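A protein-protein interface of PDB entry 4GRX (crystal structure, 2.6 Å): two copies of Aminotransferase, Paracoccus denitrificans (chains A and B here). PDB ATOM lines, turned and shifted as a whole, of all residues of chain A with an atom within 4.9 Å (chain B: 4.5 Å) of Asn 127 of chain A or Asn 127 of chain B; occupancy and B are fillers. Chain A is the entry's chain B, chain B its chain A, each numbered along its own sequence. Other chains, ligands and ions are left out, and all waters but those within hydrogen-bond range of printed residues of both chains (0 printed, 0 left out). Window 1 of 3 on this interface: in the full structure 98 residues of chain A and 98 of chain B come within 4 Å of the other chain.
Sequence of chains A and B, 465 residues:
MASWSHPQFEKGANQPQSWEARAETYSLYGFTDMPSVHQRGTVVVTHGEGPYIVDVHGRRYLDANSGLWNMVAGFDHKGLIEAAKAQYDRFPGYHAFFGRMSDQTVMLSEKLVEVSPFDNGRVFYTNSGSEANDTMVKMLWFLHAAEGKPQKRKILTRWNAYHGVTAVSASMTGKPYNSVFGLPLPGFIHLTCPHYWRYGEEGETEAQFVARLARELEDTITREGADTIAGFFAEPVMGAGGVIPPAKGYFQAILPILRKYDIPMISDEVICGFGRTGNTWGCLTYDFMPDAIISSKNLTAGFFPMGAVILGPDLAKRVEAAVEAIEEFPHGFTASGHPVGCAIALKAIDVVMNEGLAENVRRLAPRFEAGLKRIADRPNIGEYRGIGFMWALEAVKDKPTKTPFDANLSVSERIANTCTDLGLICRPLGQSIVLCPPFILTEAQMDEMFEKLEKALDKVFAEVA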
ATOM      1  N   TYR A 125     -22.278 -33.378   3.878  1.00  0.00           N
ATOM      2  CA  TYR A 125     -22.501 -32.921   2.500  1.00  0.00           C
ATOM      3  C   TYR A 125     -23.755 -32.107   2.267  1.00  0.00           C
ATOM      4  O   TYR A 125     -24.800 -32.419   2.813  1.00  0.00           O
ATOM      5  CB  TYR A 125     -22.463 -34.089   1.525  1.00  0.00           C
ATOM      6  CG  TYR A 125     -21.086 -34.694   1.401  1.00  0.00           C
ATOM      7  CD1 TYR A 125     -20.035 -33.964   0.833  1.00  0.00           C
ATOM      8  CD2 TYR A 125     -20.820 -35.977   1.866  1.00  0.00           C
ATOM      9  CE1 TYR A 125     -18.776 -34.494   0.722  1.00  0.00           C
ATOM     10  CE2 TYR A 125     -19.552 -36.523   1.745  1.00  0.00           C
ATOM     11  CZ  TYR A 125     -18.545 -35.774   1.169  1.00  0.00           C
ATOM     12  OH  TYR A 125     -17.290 -36.279   1.061  1.00  0.00           O
ATOM     13  N   THR A 126     -23.621 -31.042   1.473  1.00  0.00           N
ATOM     14  CA  THR A 126     -24.751 -30.252   0.994  1.00  0.00           C
ATOM     15  C   THR A 126     -24.658 -30.097  -0.541  1.00  0.00           C
ATOM     16  O   THR A 126     -23.735 -30.632  -1.174  1.00  0.00           O
ATOM     17  CB  THR A 126     -24.825 -28.852   1.666  1.00  0.00           C
ATOM     18  OG1 THR A 126     -23.760 -28.021   1.188  1.00  0.00           O
ATOM     19  CG2 THR A 126     -24.781 -28.939   3.221  1.00  0.00           C
ATOM     20  N   ASN A 127     -25.613 -29.375  -1.130  1.00  0.00           N
ATOM     21  CA  ASN A 127     -25.579 -29.046  -2.554  1.00  0.00           C
ATOM     22  C   ASN A 127     -24.964 -27.687  -2.867  1.00  0.00           C
ATOM     23  O   ASN A 127     -24.491 -27.462  -3.975  1.00  0.00           O
ATOM     24  CB  ASN A 127     -26.986 -29.037  -3.156  1.00  0.00           C
ATOM     25  CG  ASN A 127     -27.779 -30.286  -2.845  1.00  0.00           C
ATOM     26  OD1 ASN A 127     -27.421 -31.388  -3.262  1.00  0.00           O
ATOM     27  ND2 ASN A 127     -28.896 -30.106  -2.134  1.00  0.00           N
ATOM     28  N   SER A 128     -25.018 -26.764  -1.918  1.00  0.00           N
ATOM     29  CA  SER A 128     -24.573 -25.399  -2.166  1.00  0.00           C
ATOM     30  C   SER A 128     -23.831 -24.866  -0.948  1.00  0.00           C
ATOM     31  O   SER A 128     -23.916 -25.431   0.151  1.00  0.00           O
ATOM     32  CB  SER A 128     -25.769 -24.507  -2.499  1.00  0.00           C
ATOM     33  OG  SER A 128     -26.544 -24.231  -1.347  1.00  0.00           O
ATOM     34  N   GLY A 129     -23.097 -23.776  -1.139  1.00  0.00           N
ATOM     35  CA  GLY A 129     -22.452 -23.096  -0.020  1.00  0.00           C
ATOM     36  C   GLY A 129     -23.436 -22.507   0.970  1.00  0.00           C
ATOM     37  O   GLY A 129     -23.167 -22.503   2.173  1.00  0.00           O
ATOM     38  N   GLU A 131     -26.560 -23.664   1.598  1.00  0.00           N
ATOM     39  CA  GLU A 131     -26.999 -24.802   2.400  1.00  0.00           C
ATOM     40  C   GLU A 131     -25.981 -25.130   3.498  1.00  0.00           C
ATOM     41  O   GLU A 131     -26.358 -25.375   4.648  1.00  0.00           O
ATOM     42  CB  GLU A 131     -27.223 -26.030   1.524  1.00  0.00           C
ATOM     43  CG  GLU A 131     -28.569 -26.074   0.832  1.00  0.00           C
ATOM     44  CD  GLU A 131     -28.674 -27.229  -0.161  1.00  0.00           C
ATOM     45  OE1 GLU A 131     -27.738 -28.047  -0.255  1.00  0.00           O
ATOM     46  OE2 GLU A 131     -29.694 -27.327  -0.871  1.00  0.00           O
ATOM     47  N   PRO A 305     -23.349 -29.391  -8.545  1.00  0.00           N
ATOM     48  CA  PRO A 305     -23.653 -28.702  -7.292  1.00  0.00           C
ATOM     49  C   PRO A 305     -23.233 -29.526  -6.084  1.00  0.00           C
ATOM     50  O   PRO A 305     -23.815 -30.575  -5.818  1.00  0.00           O
ATOM     51  CB  PRO A 305     -25.170 -28.586  -7.315  1.00  0.00           C
ATOM     52  CG  PRO A 305     -25.557 -28.798  -8.728  1.00  0.00           C
ATOM     53  CD  PRO A 305     -24.571 -29.769  -9.263  1.00  0.00           C
ATOM     54  N   MET A 306     -22.229 -29.058  -5.356  1.00  0.00           N
ATOM     55  CA  MET A 306     -21.829 -29.718  -4.122  1.00  0.00           C
ATOM     56  C   MET A 306     -21.353 -28.712  -3.081  1.00  0.00           C
ATOM     57  O   MET A 306     -20.721 -27.720  -3.419  1.00  0.00           O
ATOM     58  CB  MET A 306     -20.743 -30.747  -4.405  1.00  0.00           C
ATOM     59  CG  MET A 306     -20.275 -31.514  -3.188  1.00  0.00           C
ATOM     60  SD  MET A 306     -19.847 -33.212  -3.623  1.00  0.00           S
ATOM     61  CE  MET A 306     -21.382 -33.723  -4.419  1.00  0.00           C
ATOM     62  N   GLY A 307     -21.686 -28.976  -1.819  1.00  0.00           N
ATOM     63  CA  GLY A 307     -21.212 -28.204  -0.687  1.00  0.00           C
ATOM     64  C   GLY A 307     -20.712 -29.180   0.352  1.00  0.00           C
ATOM     65  O   GLY A 307     -21.195 -30.326   0.427  1.00  0.00           O
ATOM     66  N   PHE A 333     -29.805 -33.204   3.098  1.00  0.00           N
ATOM     67  CA  PHE A 333     -30.444 -32.851   1.843  1.00  0.00           C
ATOM     68  C   PHE A 333     -30.493 -34.079   0.969  1.00  0.00           C
ATOM     69  O   PHE A 333     -29.554 -34.861   0.957  1.00  0.00           O
ATOM     70  CB  PHE A 333     -29.692 -31.714   1.148  1.00  0.00           C
ATOM     71  CG  PHE A 333     -29.561 -30.484   1.997  1.00  0.00           C
ATOM     72  CD1 PHE A 333     -30.569 -29.529   2.021  1.00  0.00           C
ATOM     73  CD2 PHE A 333     -28.431 -30.283   2.803  1.00  0.00           C
ATOM     74  CE1 PHE A 333     -30.448 -28.399   2.819  1.00  0.00           C
ATOM     75  CE2 PHE A 333     -28.319 -29.154   3.607  1.00  0.00           C
ATOM     76  CZ  PHE A 333     -29.325 -28.213   3.613  1.00  0.00           C
ATOM     77  N   ALA A 335     -30.035 -34.863  -2.103  1.00  0.00           N
ATOM     78  CA  ALA A 335     -28.876 -35.107  -2.965  1.00  0.00           C
ATOM     79  C   ALA A 335     -27.496 -35.047  -2.254  1.00  0.00           C
ATOM     80  O   ALA A 335     -26.453 -35.054  -2.916  1.00  0.00           O
ATOM     81  CB  ALA A 335     -28.912 -34.165  -4.153  1.00  0.00           C
ATOM     82  N   SER A 336     -27.495 -34.978  -0.921  1.00  0.00           N
ATOM     83  CA  SER A 336     -26.249 -34.977  -0.140  1.00  0.00           C
ATOM     84  C   SER A 336     -25.394 -36.192  -0.496  1.00  0.00           C
ATOM     85  O   SER A 336     -25.898 -37.322  -0.552  1.00  0.00           O
ATOM     86  CB  SER A 336     -26.534 -34.985   1.371  1.00  0.00           C
ATOM     87  OG  SER A 336     -26.915 -33.704   1.863  1.00  0.00           O
ATOM     88  N   THR B 126     -33.281 -23.670  -7.844  1.00  0.00           N
ATOM     89  CA  THR B 126     -32.476 -23.955  -6.665  1.00  0.00           C
ATOM     90  C   THR B 126     -31.767 -25.280  -6.866  1.00  0.00           C
ATOM     91  O   THR B 126     -31.906 -25.922  -7.920  1.00  0.00           O
ATOM     92  CB  THR B 126     -33.344 -24.091  -5.405  1.00  0.00           C
ATOM     93  OG1 THR B 126     -34.263 -25.171  -5.580  1.00  0.00           O
ATOM     94  CG2 THR B 126     -34.120 -22.832  -5.146  1.00  0.00           C
ATOM     95  N   ASN B 127     -31.032 -25.718  -5.848  1.00  0.00           N
ATOM     96  CA  ASN B 127     -30.412 -27.042  -5.909  1.00  0.00           C
ATOM     97  C   ASN B 127     -31.257 -28.110  -5.242  1.00  0.00           C
ATOM     98  O   ASN B 127     -31.341 -29.229  -5.739  1.00  0.00           O
ATOM     99  CB  ASN B 127     -29.003 -27.017  -5.324  1.00  0.00           C
ATOM    100  CG  ASN B 127     -28.091 -26.050  -6.057  1.00  0.00           C
ATOM    101  OD1 ASN B 127     -27.884 -26.172  -7.265  1.00  0.00           O
ATOM    102  ND2 ASN B 127     -27.555 -25.075  -5.335  1.00  0.00           N
ATOM    103  N   SER B 128     -31.911 -27.758  -4.140  1.00  0.00           N
ATOM    104  CA  SER B 128     -32.688 -28.718  -3.364  1.00  0.00           C
ATOM    105  C   SER B 128     -34.113 -28.247  -3.168  1.00  0.00           C
ATOM    106  O   SER B 128     -34.426 -27.083  -3.390  1.00  0.00           O
ATOM    107  CB  SER B 128     -32.030 -28.913  -2.010  1.00  0.00           C
ATOM    108  OG  SER B 128     -32.067 -27.709  -1.263  1.00  0.00           O
ATOM    109  N   GLU B 131     -34.050 -25.571  -0.226  1.00  0.00           N
ATOM    110  CA  GLU B 131     -33.740 -24.253  -0.780  1.00  0.00           C
ATOM    111  C   GLU B 131     -34.954 -23.611  -1.458  1.00  0.00           C
ATOM    112  O   GLU B 131     -35.206 -22.441  -1.254  1.00  0.00           O
ATOM    113  CB  GLU B 131     -32.604 -24.350  -1.789  1.00  0.00           C
ATOM    114  CG  GLU B 131     -31.212 -24.409  -1.190  1.00  0.00           C
ATOM    115  CD  GLU B 131     -30.086 -24.548  -2.231  1.00  0.00           C
ATOM    116  OE1 GLU B 131     -30.251 -25.235  -3.257  1.00  0.00           O
ATOM    117  OE2 GLU B 131     -28.996 -23.989  -2.006  1.00  0.00           O
ATOM    118  N   PRO B 305     -28.871 -32.600  -8.747  1.00  0.00           N
ATOM    119  CA  PRO B 305     -29.549 -31.738  -7.758  1.00  0.00           C
ATOM    120  C   PRO B 305     -30.278 -30.530  -8.374  1.00  0.00           C
ATOM    121  O   PRO B 305     -29.651 -29.594  -8.856  1.00  0.00           O
ATOM    122  CB  PRO B 305     -28.403 -31.268  -6.837  1.00  0.00           C
ATOM    123  CG  PRO B 305     -27.235 -32.119  -7.178  1.00  0.00           C
ATOM    124  CD  PRO B 305     -27.411 -32.526  -8.610  1.00  0.00           C
ATOM    125  N   MET B 306     -31.601 -30.546  -8.338  1.00  0.00           N
ATOM    126  CA  MET B 306     -32.375 -29.489  -8.957  1.00  0.00           C
ATOM    127  C   MET B 306     -33.610 -29.191  -8.138  1.00  0.00           C
ATOM    128  O   MET B 306     -34.269 -30.107  -7.639  1.00  0.00           O
ATOM    129  CB  MET B 306     -32.821 -29.934 -10.339  1.00  0.00           C
ATOM    130  CG  MET B 306     -33.264 -28.819 -11.264  1.00  0.00           C
ATOM    131  SD  MET B 306     -31.901 -28.245 -12.295  1.00  0.00           S
ATOM    132  CE  MET B 306     -32.874 -27.528 -13.604  1.00  0.00           C
ATOM    133  N   GLY B 307     -33.916 -27.905  -8.012  1.00  0.00           N
ATOM    134  CA  GLY B 307     -35.181 -27.440  -7.455  1.00  0.00           C
ATOM    135  C   GLY B 307     -35.793 -26.350  -8.316  1.00  0.00           C
ATOM    136  O   GLY B 307     -35.088 -25.612  -9.009  1.00  0.00           O
ATOM    137  N   PHE B 333     -28.679 -19.013  -6.067  1.00  0.00           N
ATOM    138  CA  PHE B 333     -27.636 -19.991  -5.705  1.00  0.00           C
ATOM    139  C   PHE B 333     -26.651 -20.206  -6.866  1.00  0.00           C
ATOM    140  O   PHE B 333     -27.055 -20.201  -8.032  1.00  0.00           O
ATOM    141  CB  PHE B 333     -28.277 -21.332  -5.297  1.00  0.00           C
ATOM    142  CG  PHE B 333     -29.403 -21.196  -4.297  1.00  0.00           C
ATOM    143  CD1 PHE B 333     -29.143 -21.190  -2.924  1.00  0.00           C
ATOM    144  CD2 PHE B 333     -30.725 -21.064  -4.722  1.00  0.00           C
ATOM    145  CE1 PHE B 333     -30.178 -21.057  -1.994  1.00  0.00           C
ATOM    146  CE2 PHE B 333     -31.758 -20.929  -3.800  1.00  0.00           C
ATOM    147  CZ  PHE B 333     -31.487 -20.926  -2.434  1.00  0.00           C
ATOM    148  N   ALA B 335     -25.133 -22.672  -8.373  1.00  0.00           N
ATOM    149  CA  ALA B 335     -25.417 -23.701  -9.374  1.00  0.00           C
ATOM    150  C   ALA B 335     -26.871 -23.702  -9.879  1.00  0.00           C
ATOM    151  O   ALA B 335     -27.251 -24.566 -10.676  1.00  0.00           O
ATOM    152  CB  ALA B 335     -25.031 -25.073  -8.837  1.00  0.00           C
ATOM    153  N   SER B 336     -27.678 -22.737  -9.432  1.00  0.00           N
ATOM    154  CA  SER B 336     -29.083 -22.685  -9.851  1.00  0.00           C
ATOM    155  C   SER B 336     -29.228 -22.299 -11.342  1.00  0.00           C
ATOM    156  O   SER B 336     -28.601 -21.330 -11.819  1.00  0.00           O
ATOM    157  CB  SER B 336     -29.927 -21.810  -8.901  1.00  0.00           C
ATOM    158  OG  SER B 336     -29.794 -20.417  -9.141  1.00  0.00           O
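The side-chain hydroxyl (OG) of Ser 128 of chain A is in hydrogen-bond range of the side-chain carboxylate (OE2) of Glu 131 of chain B (2.6 Å). OE2 of Glu 131 of chain A lies close to OE1 of Glu 131 of chain B (3.2 Å). The side-chain hydroxyl of Ser 128 of chain B is in hydrogen-bond range of the side-chain carboxylate of Glu 131 of chain A (2.4 Å).
The backbone carbonyl oxygen (O) of Ser 128 of chain A lies within hydrogen-bond range of the side-chain hydroxyl (OG1) of Thr 126 of chain A (2.8 Å). OG of Ser 128 of chain A sits at hydrogen-bond distance from N of Glu 131 of chain A, 3.0 Å away. N of Met 306 of chain B is in hydrogen-bond range of O of Asn 127 of chain B, at 2.9 Å. The side-chain hydroxyl of Thr 126 of chain B lies within hydrogen-bond range of the backbone carbonyl oxygen of Ser 128 of chain B (2.9 Å). The backbone NH of Asn 127 of chain B lies within hydrogen-bond range of the side-chain carboxylate of Glu 131 of chain B, 2.7 Å away. The backbone NH (N) of Met 306 of chain A sits at hydrogen-bond distance from the backbone carbonyl oxygen (O) of Asn 127 of chain A (3.1 Å).
Among the printed residues, merely in contact across the chains: Asn 127 of chain A with Ser 128 of chain B (3.4 Å), Ser 128 of chain A with Asn 127 of chain B (3.4 Å), Asn 127 of chain A with Asn 127 of chain B (3.6 Å), Pro 305 of chain A with Asn 127 of chain B (3.6 Å), Asn 127 of chain A with Pro 305 of chain B (3.7 Å), Pro 305 of chain A with Ala 335 of chain B (3.8 Å), Ala 335 of chain A with Pro 305 of chain B (3.98 Å) and Pro 305 of chain A with Pro 305 of chain B (3.99 Å).
Of chain B, only Asn 127, Ser 128 and Pro 305 come within 4 Å of Asn 127 of chain A. Printed residues of chain B within 4 Å of Ser 128 of chain A: Asn 127 (3.4 Å) and Glu 131 (2.6 Å). Printed residues of chain B within 4 Å of Pro 305 of chain A: Asn 127, Pro 305 and Ala 335. Phe 333 of chain A touches none of the printed residues of chain B. Of chain A, only Asn 127, Ser 128 and Pro 305 come within 4 Å of Asn 127 of chain B.
Of the 12 printed residues of chain A, 5 touch a printed residue of chain B. Hydrophobic or aromatic side chains of chain A that line the printed part of chain B: Pro 305 and Ala 335. Among the printed residues, 11 pairs touch across the chains.
Asn 127 of chain A touches its own counterpart, Asn 127 of chain B. Asn 127 of chain A touches Ser 128 of chain B, and with the chains exchanged Ser 128 of chain A touches Asn 127 of chain B. Ser 128 of chain A touches Glu 131 of chain B, and with the chains exchanged Glu 131 of chain A touches Ser 128 of chain B. Glu 131 of chain B touches its own counterpart, Glu 131 of chain A.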
